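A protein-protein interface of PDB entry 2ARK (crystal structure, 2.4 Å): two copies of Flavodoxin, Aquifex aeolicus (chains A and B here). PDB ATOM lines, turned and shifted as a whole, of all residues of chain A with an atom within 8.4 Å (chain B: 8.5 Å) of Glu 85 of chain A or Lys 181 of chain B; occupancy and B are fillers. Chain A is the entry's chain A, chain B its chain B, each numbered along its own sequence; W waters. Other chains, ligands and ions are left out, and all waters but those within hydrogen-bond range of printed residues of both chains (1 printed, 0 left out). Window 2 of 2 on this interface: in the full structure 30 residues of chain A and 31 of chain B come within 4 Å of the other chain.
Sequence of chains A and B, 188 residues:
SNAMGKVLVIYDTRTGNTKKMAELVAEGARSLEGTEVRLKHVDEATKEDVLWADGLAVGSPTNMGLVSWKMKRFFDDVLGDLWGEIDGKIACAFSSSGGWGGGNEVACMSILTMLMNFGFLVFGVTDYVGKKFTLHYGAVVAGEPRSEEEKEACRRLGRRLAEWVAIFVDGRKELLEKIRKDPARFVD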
ATOM      1  N   LYS A  47      17.258 -34.197   1.640  1.00  0.00           N
ATOM      2  CA  LYS A  47      17.641 -33.438   2.818  1.00  0.00           C
ATOM      3  C   LYS A  47      17.162 -34.129   4.105  1.00  0.00           C
ATOM      4  O   LYS A  47      17.769 -33.966   5.134  1.00  0.00           O
ATOM      5  CB  LYS A  47      17.205 -31.949   2.714  1.00  0.00           C
ATOM      6  CG  LYS A  47      15.727 -31.620   3.002  1.00  0.00           C
ATOM      7  CD  LYS A  47      15.440 -30.114   2.746  1.00  0.00           C
ATOM      8  CE  LYS A  47      14.252 -29.542   3.554  1.00  0.00           C
ATOM      9  NZ  LYS A  47      12.861 -29.938   3.136  1.00  0.00           N
ATOM     10  N   LEU A  51      19.144 -35.127   7.727  1.00  0.00           N
ATOM     11  CA  LEU A  51      18.518 -34.833   9.016  1.00  0.00           C
ATOM     12  C   LEU A  51      18.355 -36.068   9.912  1.00  0.00           C
ATOM     13  O   LEU A  51      18.477 -35.995  11.127  1.00  0.00           O
ATOM     14  CB  LEU A  51      17.154 -34.192   8.779  1.00  0.00           C
ATOM     15  CG  LEU A  51      17.194 -32.757   8.279  1.00  0.00           C
ATOM     16  CD1 LEU A  51      15.827 -32.374   7.697  1.00  0.00           C
ATOM     17  CD2 LEU A  51      17.603 -31.829   9.434  1.00  0.00           C
ATOM     18  N   LEU A  79      21.120 -29.358   0.395  1.00  0.00           N
ATOM     19  CA  LEU A  79      21.393 -29.109   1.811  1.00  0.00           C
ATOM     20  C   LEU A  79      21.572 -27.640   2.176  1.00  0.00           C
ATOM     21  O   LEU A  79      21.633 -27.295   3.349  1.00  0.00           O
ATOM     22  CB  LEU A  79      22.599 -29.901   2.281  1.00  0.00           C
ATOM     23  CG  LEU A  79      22.563 -31.416   2.155  1.00  0.00           C
ATOM     24  CD1 LEU A  79      23.696 -31.914   2.973  1.00  0.00           C
ATOM     25  CD2 LEU A  79      21.215 -32.026   2.658  1.00  0.00           C
ATOM     26  N   GLY A  80      21.631 -26.779   1.176  1.00  0.00           N
ATOM     27  CA  GLY A  80      21.861 -25.355   1.402  1.00  0.00           C
ATOM     28  C   GLY A  80      20.940 -24.656   2.392  1.00  0.00           C
ATOM     29  O   GLY A  80      21.370 -23.719   3.068  1.00  0.00           O
ATOM     30  N   ASP A  81      19.677 -25.090   2.469  1.00  0.00           N
ATOM     31  CA  ASP A  81      18.722 -24.538   3.447  1.00  0.00           C
ATOM     32  C   ASP A  81      18.975 -25.022   4.861  1.00  0.00           C
ATOM     33  O   ASP A  81      18.659 -24.340   5.804  1.00  0.00           O
ATOM     34  CB  ASP A  81      17.260 -24.822   3.047  1.00  0.00           C
ATOM     35  CG  ASP A  81      16.705 -23.786   2.042  1.00  0.00           C
ATOM     36  OD1 ASP A  81      15.687 -24.079   1.361  1.00  0.00           O
ATOM     37  OD2 ASP A  81      17.277 -22.671   1.927  1.00  0.00           O
ATOM     38  N   LEU A  82      19.539 -26.209   4.998  1.00  0.00           N
ATOM     39  CA  LEU A  82      19.887 -26.763   6.307  1.00  0.00           C
ATOM     40  C   LEU A  82      21.176 -26.176   6.893  1.00  0.00           C
ATOM     41  O   LEU A  82      21.508 -26.443   8.049  1.00  0.00           O
ATOM     42  CB  LEU A  82      20.019 -28.285   6.208  1.00  0.00           C
ATOM     43  CG  LEU A  82      18.743 -29.086   5.920  1.00  0.00           C
ATOM     44  CD1 LEU A  82      19.070 -30.570   5.994  1.00  0.00           C
ATOM     45  CD2 LEU A  82      17.608 -28.717   6.877  1.00  0.00           C
ATOM     46  N   TRP A  83      21.892 -25.385   6.094  1.00  0.00           N
ATOM     47  CA  TRP A  83      23.217 -24.942   6.461  1.00  0.00           C
ATOM     48  C   TRP A  83      23.066 -24.053   7.681  1.00  0.00           C
ATOM     49  O   TRP A  83      22.259 -23.102   7.688  1.00  0.00           O
ATOM     50  CB  TRP A  83      23.940 -24.208   5.313  1.00  0.00           C
ATOM     51  CG  TRP A  83      25.383 -23.813   5.675  1.00  0.00           C
ATOM     52  CD1 TRP A  83      26.512 -24.529   5.434  1.00  0.00           C
ATOM     53  CD2 TRP A  83      25.814 -22.634   6.384  1.00  0.00           C
ATOM     54  NE1 TRP A  83      27.617 -23.878   5.931  1.00  0.00           N
ATOM     55  CE2 TRP A  83      27.220 -22.712   6.515  1.00  0.00           C
ATOM     56  CE3 TRP A  83      25.148 -21.522   6.918  1.00  0.00           C
ATOM     57  CZ2 TRP A  83      27.979 -21.719   7.139  1.00  0.00           C
ATOM     58  CZ3 TRP A  83      25.907 -20.533   7.553  1.00  0.00           C
ATOM     59  CH2 TRP A  83      27.311 -20.642   7.650  1.00  0.00           C
ATOM     60  N   GLY A  84      23.832 -24.390   8.722  1.00  0.00           N
ATOM     61  CA  GLY A  84      23.866 -23.583   9.925  1.00  0.00           C
ATOM     62  C   GLY A  84      23.018 -24.181  11.014  1.00  0.00           C
ATOM     63  O   GLY A  84      23.145 -23.788  12.145  1.00  0.00           O
ATOM     64  N   GLU A  85      22.161 -25.142  10.684  1.00  0.00           N
ATOM     65  CA  GLU A  85      21.289 -25.723  11.703  1.00  0.00           C
ATOM     66  C   GLU A  85      21.482 -27.236  11.839  1.00  0.00           C
ATOM     67  O   GLU A  85      20.673 -27.914  12.479  1.00  0.00           O
ATOM     68  CB  GLU A  85      19.812 -25.365  11.456  1.00  0.00           C
ATOM     69  CG  GLU A  85      19.164 -26.212  10.342  1.00  0.00           C
ATOM     70  CD  GLU A  85      17.655 -25.960  10.151  1.00  0.00           C
ATOM     71  OE1 GLU A  85      16.913 -25.913  11.152  1.00  0.00           O
ATOM     72  OE2 GLU A  85      17.212 -25.811   8.986  1.00  0.00           O
ATOM     73  N   ILE A  86      22.543 -27.769  11.253  1.00  0.00           N
ATOM     74  CA  ILE A  86      22.818 -29.199  11.392  1.00  0.00           C
ATOM     75  C   ILE A  86      24.236 -29.494  11.867  1.00  0.00           C
ATOM     76  O   ILE A  86      24.749 -30.561  11.587  1.00  0.00           O
ATOM     77  CB  ILE A  86      22.483 -30.038  10.100  1.00  0.00           C
ATOM     78  CG1 ILE A  86      23.229 -29.505   8.882  1.00  0.00           C
ATOM     79  CG2 ILE A  86      20.980 -30.064   9.853  1.00  0.00           C
ATOM     80  CD1 ILE A  86      23.113 -30.359   7.672  1.00  0.00           C
ATOM     81  N   ASP A  87      24.848 -28.554  12.594  1.00  0.00           N
ATOM     82  CA  ASP A  87      26.206 -28.704  13.122  1.00  0.00           C
ATOM     83  C   ASP A  87      26.341 -29.909  14.027  1.00  0.00           C
ATOM     84  O   ASP A  87      25.400 -30.263  14.729  1.00  0.00           O
ATOM     85  CB  ASP A  87      26.605 -27.477  13.927  1.00  0.00           C
ATOM     86  CG  ASP A  87      26.642 -26.194  13.099  1.00  0.00           C
ATOM     87  OD1 ASP A  87      25.612 -25.829  12.491  1.00  0.00           O
ATOM     88  OD2 ASP A  87      27.705 -25.543  13.084  1.00  0.00           O
ATOM     89  N   GLY A  88      27.519 -30.534  14.014  1.00  0.00           N
ATOM     90  CA  GLY A  88      27.813 -31.613  14.956  1.00  0.00           C
ATOM     91  C   GLY A  88      27.389 -33.006  14.515  1.00  0.00           C
ATOM     92  O   GLY A  88      27.414 -33.941  15.313  1.00  0.00           O
ATOM     93  N   LYS A  89      26.983 -33.152  13.254  1.00  0.00           N
ATOM     94  CA  LYS A  89      26.891 -34.479  12.660  1.00  0.00           C
ATOM     95  C   LYS A  89      28.308 -34.944  12.479  1.00  0.00           C
ATOM     96  O   LYS A  89      29.216 -34.114  12.409  1.00  0.00           O
ATOM     97  CB  LYS A  89      26.119 -34.486  11.334  1.00  0.00           C
ATOM     98  CG  LYS A  89      24.632 -34.504  11.546  1.00  0.00           C
ATOM     99  CD  LYS A  89      23.854 -34.360  10.260  1.00  0.00           C
ATOM    100  CE  LYS A  89      22.482 -33.781  10.579  1.00  0.00           C
ATOM    101  NZ  LYS A  89      21.734 -34.641  11.525  1.00  0.00           N
ATOM    102  N   PHE A 118      29.734 -27.413   6.869  1.00  0.00           N
ATOM    103  CA  PHE A 118      28.430 -27.538   7.509  1.00  0.00           C
ATOM    104  C   PHE A 118      28.527 -27.708   9.025  1.00  0.00           C
ATOM    105  O   PHE A 118      27.523 -27.998   9.674  1.00  0.00           O
ATOM    106  CB  PHE A 118      27.650 -28.715   6.915  1.00  0.00           C
ATOM    107  CG  PHE A 118      26.926 -28.389   5.634  1.00  0.00           C
ATOM    108  CD1 PHE A 118      27.577 -28.485   4.402  1.00  0.00           C
ATOM    109  CD2 PHE A 118      25.586 -28.005   5.663  1.00  0.00           C
ATOM    110  CE1 PHE A 118      26.909 -28.204   3.207  1.00  0.00           C
ATOM    111  CE2 PHE A 118      24.894 -27.707   4.482  1.00  0.00           C
ATOM    112  CZ  PHE A 118      25.569 -27.821   3.241  1.00  0.00           C
ATOM    113  N   GLY A 119      29.725 -27.550   9.578  1.00  0.00           N
ATOM    114  CA  GLY A 119      29.927 -27.621  10.984  1.00  0.00           C
ATOM    115  C   GLY A 119      29.959 -29.037  11.513  1.00  0.00           C
ATOM    116  O   GLY A 119      29.831 -29.246  12.733  1.00  0.00           O
ATOM    117  N   PHE A 120      30.124 -30.011  10.611  1.00  0.00           N
ATOM    118  CA  PHE A 120      30.265 -31.417  10.998  1.00  0.00           C
ATOM    119  C   PHE A 120      31.631 -31.684  11.637  1.00  0.00           C
ATOM    120  O   PHE A 120      32.607 -30.976  11.383  1.00  0.00           O
ATOM    121  CB  PHE A 120      30.097 -32.345   9.786  1.00  0.00           C
ATOM    122  CG  PHE A 120      28.753 -32.253   9.103  1.00  0.00           C
ATOM    123  CD1 PHE A 120      27.687 -31.557   9.681  1.00  0.00           C
ATOM    124  CD2 PHE A 120      28.549 -32.919   7.902  1.00  0.00           C
ATOM    125  CE1 PHE A 120      26.449 -31.509   9.073  1.00  0.00           C
ATOM    126  CE2 PHE A 120      27.313 -32.902   7.259  1.00  0.00           C
ATOM    127  CZ  PHE A 120      26.247 -32.183   7.840  1.00  0.00           C
ATOM    128  N   THR B 126      30.634 -22.691  11.862  1.00  0.00           N
ATOM    129  CA  THR B 126      29.721 -22.050  10.919  1.00  0.00           C
ATOM    130  C   THR B 126      29.419 -20.598  11.292  1.00  0.00           C
ATOM    131  O   THR B 126      29.280 -19.750  10.399  1.00  0.00           O
ATOM    132  CB  THR B 126      28.380 -22.802  10.836  1.00  0.00           C
ATOM    133  OG1 THR B 126      27.912 -23.103  12.162  1.00  0.00           O
ATOM    134  CG2 THR B 126      28.521 -24.072  10.046  1.00  0.00           C
ATOM    135  N   ASP B 127      29.327 -20.352  12.606  1.00  0.00           N
ATOM    136  CA  ASP B 127      28.955 -19.078  13.217  1.00  0.00           C
ATOM    137  C   ASP B 127      29.575 -17.889  12.533  1.00  0.00           C
ATOM    138  O   ASP B 127      30.790 -17.865  12.305  1.00  0.00           O
ATOM    139  CB  ASP B 127      29.374 -19.013  14.698  1.00  0.00           C
ATOM    140  CG  ASP B 127      28.643 -20.022  15.588  1.00  0.00           C
ATOM    141  OD1 ASP B 127      28.115 -21.007  15.051  1.00  0.00           O
ATOM    142  OD2 ASP B 127      28.639 -19.851  16.849  1.00  0.00           O
ATOM    143  N   LEU B 175      22.187 -29.641  24.715  1.00  0.00           N
ATOM    144  CA  LEU B 175      22.893 -28.466  24.191  1.00  0.00           C
ATOM    145  C   LEU B 175      22.873 -28.423  22.677  1.00  0.00           C
ATOM    146  O   LEU B 175      22.915 -27.333  22.106  1.00  0.00           O
ATOM    147  CB  LEU B 175      24.358 -28.379  24.630  1.00  0.00           C
ATOM    148  CG  LEU B 175      24.860 -28.253  26.058  1.00  0.00           C
ATOM    149  CD1 LEU B 175      26.331 -27.812  25.975  1.00  0.00           C
ATOM    150  CD2 LEU B 175      24.013 -27.292  26.935  1.00  0.00           C
ATOM    151  N   LEU B 176      22.840 -29.602  22.043  1.00  0.00           N
ATOM    152  CA  LEU B 176      22.936 -29.726  20.582  1.00  0.00           C
ATOM    153  C   LEU B 176      21.874 -28.911  19.841  1.00  0.00           C
ATOM    154  O   LEU B 176      22.210 -28.096  18.950  1.00  0.00           O
ATOM    155  CB  LEU B 176      22.913 -31.197  20.138  1.00  0.00           C
ATOM    156  CG  LEU B 176      23.176 -31.491  18.651  1.00  0.00           C
ATOM    157  CD1 LEU B 176      24.480 -30.832  18.129  1.00  0.00           C
ATOM    158  CD2 LEU B 176      23.162 -32.999  18.346  1.00  0.00           C
ATOM    159  N   GLU B 177      20.610 -29.120  20.210  1.00  0.00           N
ATOM    160  CA  GLU B 177      19.495 -28.446  19.553  1.00  0.00           C
ATOM    161  C   GLU B 177      19.455 -26.965  19.908  1.00  0.00           C
ATOM    162  O   GLU B 177      19.013 -26.143  19.106  1.00  0.00           O
ATOM    163  CB  GLU B 177      18.162 -29.128  19.907  1.00  0.00           C
ATOM    164  CG  GLU B 177      16.930 -28.569  19.189  1.00  0.00           C
ATOM    165  CD  GLU B 177      17.012 -28.680  17.652  1.00  0.00           C
ATOM    166  OE1 GLU B 177      16.210 -27.974  16.984  1.00  0.00           O
ATOM    167  OE2 GLU B 177      17.866 -29.461  17.125  1.00  0.00           O
ATOM    168  N   LYS B 178      19.913 -26.640  21.115  1.00  0.00           N
ATOM    169  CA  LYS B 178      20.012 -25.249  21.578  1.00  0.00           C
ATOM    170  C   LYS B 178      21.018 -24.439  20.746  1.00  0.00           C
ATOM    171  O   LYS B 178      20.744 -23.295  20.361  1.00  0.00           O
ATOM    172  CB  LYS B 178      20.302 -25.187  23.095  1.00  0.00           C
ATOM    173  CG  LYS B 178      19.100 -25.694  23.925  1.00  0.00           C
ATOM    174  CD  LYS B 178      19.129 -25.335  25.426  1.00  0.00           C
ATOM    175  CE  LYS B 178      17.870 -25.926  26.109  1.00  0.00           C
ATOM    176  NZ  LYS B 178      17.645 -25.456  27.516  1.00  0.00           N
ATOM    177  N   ILE B 179      22.166 -25.053  20.460  1.00  0.00           N
ATOM    178  CA  ILE B 179      23.174 -24.470  19.592  1.00  0.00           C
ATOM    179  C   ILE B 179      22.615 -24.355  18.175  1.00  0.00           C
ATOM    180  O   ILE B 179      22.729 -23.301  17.545  1.00  0.00           O
ATOM    181  CB  ILE B 179      24.486 -25.315  19.596  1.00  0.00           C
ATOM    182  CG1 ILE B 179      25.158 -25.249  20.970  1.00  0.00           C
ATOM    183  CG2 ILE B 179      25.448 -24.840  18.533  1.00  0.00           C
ATOM    184  CD1 ILE B 179      26.159 -26.364  21.205  1.00  0.00           C
ATOM    185  N   ARG B 180      21.999 -25.433  17.680  1.00  0.00           N
ATOM    186  CA  ARG B 180      21.554 -25.471  16.283  1.00  0.00           C
ATOM    187  C   ARG B 180      20.567 -24.367  15.920  1.00  0.00           C
ATOM    188  O   ARG B 180      20.615 -23.820  14.798  1.00  0.00           O
ATOM    189  CB  ARG B 180      21.003 -26.855  15.898  1.00  0.00           C
ATOM    190  CG  ARG B 180      22.101 -27.885  15.654  1.00  0.00           C
ATOM    191  CD  ARG B 180      21.516 -29.255  15.538  1.00  0.00           C
ATOM    192  NE  ARG B 180      22.463 -30.230  15.012  1.00  0.00           N
ATOM    193  CZ  ARG B 180      22.195 -31.523  14.837  1.00  0.00           C
ATOM    194  NH1 ARG B 180      21.004 -32.019  15.161  1.00  0.00           N
ATOM    195  NH2 ARG B 180      23.120 -32.320  14.336  1.00  0.00           N
ATOM    196  N   LYS B 181      19.707 -24.028  16.881  1.00  0.00           N
ATOM    197  CA  LYS B 181      18.599 -23.114  16.643  1.00  0.00           C
ATOM    198  C   LYS B 181      18.859 -21.722  17.238  1.00  0.00           C
ATOM    199  O   LYS B 181      17.965 -20.880  17.271  1.00  0.00           O
ATOM    200  CB  LYS B 181      17.253 -23.754  17.099  1.00  0.00           C
ATOM    201  CG  LYS B 181      16.425 -24.506  15.977  1.00  0.00           C
ATOM    202  CD  LYS B 181      17.229 -25.610  15.237  1.00  0.00           C
ATOM    203  CE  LYS B 181      16.547 -26.223  13.993  1.00  0.00           C
ATOM    204  NZ  LYS B 181      15.394 -27.196  14.208  1.00  0.00           N
ATOM    205  N   ASP B 182      20.093 -21.469  17.683  1.00  0.00           N
ATOM    206  CA  ASP B 182      20.438 -20.193  18.324  1.00  0.00           C
ATOM    207  C   ASP B 182      20.716 -19.094  17.291  1.00  0.00           C
ATOM    208  O   ASP B 182      21.711 -19.176  16.565  1.00  0.00           O
ATOM    209  CB  ASP B 182      21.620 -20.359  19.279  1.00  0.00           C
ATOM    210  CG  ASP B 182      22.148 -19.015  19.847  1.00  0.00           C
ATOM    211  OD1 ASP B 182      23.313 -18.957  20.275  1.00  0.00           O
ATOM    212  OD2 ASP B 182      21.424 -18.015  19.868  1.00  0.00           O
ATOM    213  N   PRO B 183      19.827 -18.055  17.230  1.00  0.00           N
ATOM    214  CA  PRO B 183      19.935 -16.933  16.275  1.00  0.00           C
ATOM    215  C   PRO B 183      21.184 -16.095  16.461  1.00  0.00           C
ATOM    216  O   PRO B 183      21.654 -15.491  15.496  1.00  0.00           O
ATOM    217  CB  PRO B 183      18.698 -16.076  16.574  1.00  0.00           C
ATOM    218  CG  PRO B 183      17.765 -16.980  17.317  1.00  0.00           C
ATOM    219  CD  PRO B 183      18.641 -17.902  18.104  1.00  0.00           C
ATOM    220  N   ALA B 184      21.716 -16.068  17.683  1.00  0.00           N
ATOM    221  CA  ALA B 184      22.882 -15.263  18.014  1.00  0.00           C
ATOM    222  C   ALA B 184      24.168 -15.767  17.364  1.00  0.00           C
ATOM    223  O   ALA B 184      25.191 -15.081  17.373  1.00  0.00           O
ATOM    224  CB  ALA B 184      23.055 -15.151  19.550  1.00  0.00           C
ATOM    225  N   ARG B 185      24.126 -16.965  16.805  1.00  0.00           N
ATOM    226  CA  ARG B 185      25.297 -17.540  16.192  1.00  0.00           C
ATOM    227  C   ARG B 185      25.626 -16.833  14.875  1.00  0.00           C
ATOM    228  O   ARG B 185      26.715 -17.011  14.321  1.00  0.00           O
ATOM    229  CB  ARG B 185      25.081 -19.034  15.980  1.00  0.00           C
ATOM    230  CG  ARG B 185      25.154 -19.891  17.261  1.00  0.00           C
ATOM    231  CD  ARG B 185      24.827 -21.362  16.956  1.00  0.00           C
ATOM    232  NE  ARG B 185      25.556 -21.816  15.771  1.00  0.00           N
ATOM    233  CZ  ARG B 185      25.070 -22.604  14.824  1.00  0.00           C
ATOM    234  NH1 ARG B 185      25.837 -22.913  13.797  1.00  0.00           N
ATOM    235  NH2 ARG B 185      23.826 -23.068  14.894  1.00  0.00           N
ATOM    236  N   PHE B 186      24.692 -16.017  14.384  1.00  0.00           N
ATOM    237  CA  PHE B 186      24.842 -15.349  13.083  1.00  0.00           C
ATOM    238  C   PHE B 186      24.572 -13.859  13.166  1.00  0.00           C
ATOM    239  O   PHE B 186      23.425 -13.429  13.222  1.00  0.00           O
ATOM    240  CB  PHE B 186      24.003 -16.052  11.974  1.00  0.00           C
ATOM    241  CG  PHE B 186      24.385 -17.490  11.789  1.00  0.00           C
ATOM    242  CD1 PHE B 186      23.719 -18.502  12.496  1.00  0.00           C
ATOM    243  CD2 PHE B 186      25.482 -17.833  10.998  1.00  0.00           C
ATOM    244  CE1 PHE B 186      24.123 -19.836  12.384  1.00  0.00           C
ATOM    245  CE2 PHE B 186      25.894 -19.175  10.882  1.00  0.00           C
ATOM    246  CZ  PHE B 186      25.218 -20.167  11.569  1.00  0.00           C
HETATM  247  O   HOH W   1      22.236 -35.018  14.150  1.00  0.00           O
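The backbone carbonyl oxygen (O) of Gly 84 of chain A sits at hydrogen-bond distance from the guanidinium group (NH2) of Arg 185 of chain B. The side-chain amino group (NZ) of Lys 181 of chain B lies within salt-bridge range of the side-chain carboxylate (OE1) of Glu 85 of chain A (3.6 Å). OD2 of Asp 87 of chain A is in hydrogen-bond range of OG1 of Thr 126 of chain B (2.6 Å). O of Asp 87 of chain A is in hydrogen-bond range of NE of Arg 180 of chain B. NH1 of Arg 185 of chain B is in salt-bridge range of OD1 of Asp 87 of chain A, at 3.2 Å.
The backbone NH of Gly 88 of chain A sits at hydrogen-bond distance from the backbone carbonyl oxygen of Gly 119 of chain A. The side-chain hydroxyl (OG1) of Thr 126 of chain B is in hydrogen-bond range of the guanidinium group (NH1) of Arg 185 of chain B (2.6 Å). The side-chain carboxylate (OD1) of Asp 127 of chain B lies within salt-bridge range of the guanidinium group (NE) of Arg 185 of chain B, at 2.8 Å. OE1 of Glu 177 of chain B lies within salt-bridge range of NZ of Lys 181 of chain B (3.0 Å). The guanidinium group (NH2) of Arg 185 of chain B is in hydrogen-bond range of the backbone carbonyl oxygen (O) of Ile 179 of chain B (2.9 Å). O of Arg 180 of chain B lies within hydrogen-bond range of NH2 of Arg 185 of chain B, at 3.3 Å.
Among the printed residues, merely in contact across the chains: Glu 85 of chain A with Arg 180 of chain B (3.4 Å), Trp 83 of chain A with Thr 126 of chain B (3.5 Å), Asp 87 of chain A with Leu 176 of chain B (3.6 Å), Trp 83 of chain A with Phe 186 of chain B (3.6 Å), Ile 86 of chain A with Arg 180 of chain B (3.6 Å), Gly 84 of chain A with Arg 180 of chain B (3.7 Å), Gly 119 of chain A with Thr 126 of chain B (3.7 Å), Phe 118 of chain A with Thr 126 of chain B (3.8 Å) and Lys 89 of chain A with Arg 180 of chain B (3.9 Å).
Glu 85 of chain A touches just these residues of chain B: Arg 180 (3.4 Å) and Lys 181 (2.9 Å). Lys 181 of chain B touches just one residue of chain A: Glu 85 (2.9 Å). Of chain B, only Arg 180 and Arg 185 come within 4 Å of Gly 84 of chain A. Printed residues of chain B within 4 Å of Lys 89 of chain A: Arg 180 (3.9 Å). Of the printed residues of chain A, Arg 185 of chain B touches Gly 84 and Asp 87. The nearest residue of chain B that does not touch Glu 85 of chain A is Arg 185 of chain B (4.9 Å). The nearest printed residue of chain B that does not touch Gly 119 of chain A is Arg 185 of chain B (6.8 Å).
Printed residues of chain A that touch a printed residue of chain B: Trp 83, Gly 84, Glu 85, Ile 86, Asp 87, Lys 89, Phe 118 and Gly 119. Hydrophobic or aromatic side chains of chain A within 4 Å of the printed part of chain B: Trp 83. Hydrophobic or aromatic side chains of chain B within 4 Å of the printed part of chain A: Leu 176 and Phe 186. Among the printed residues, 14 pairs touch across the chains.
No position is printed for both chains.
Water W1 bridges the side-chain amino group (NZ) of Lys 89 of chain A (2.7 Å) and the guanidinium group (NH2) of Arg 180 of chain B (2.8 Å).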
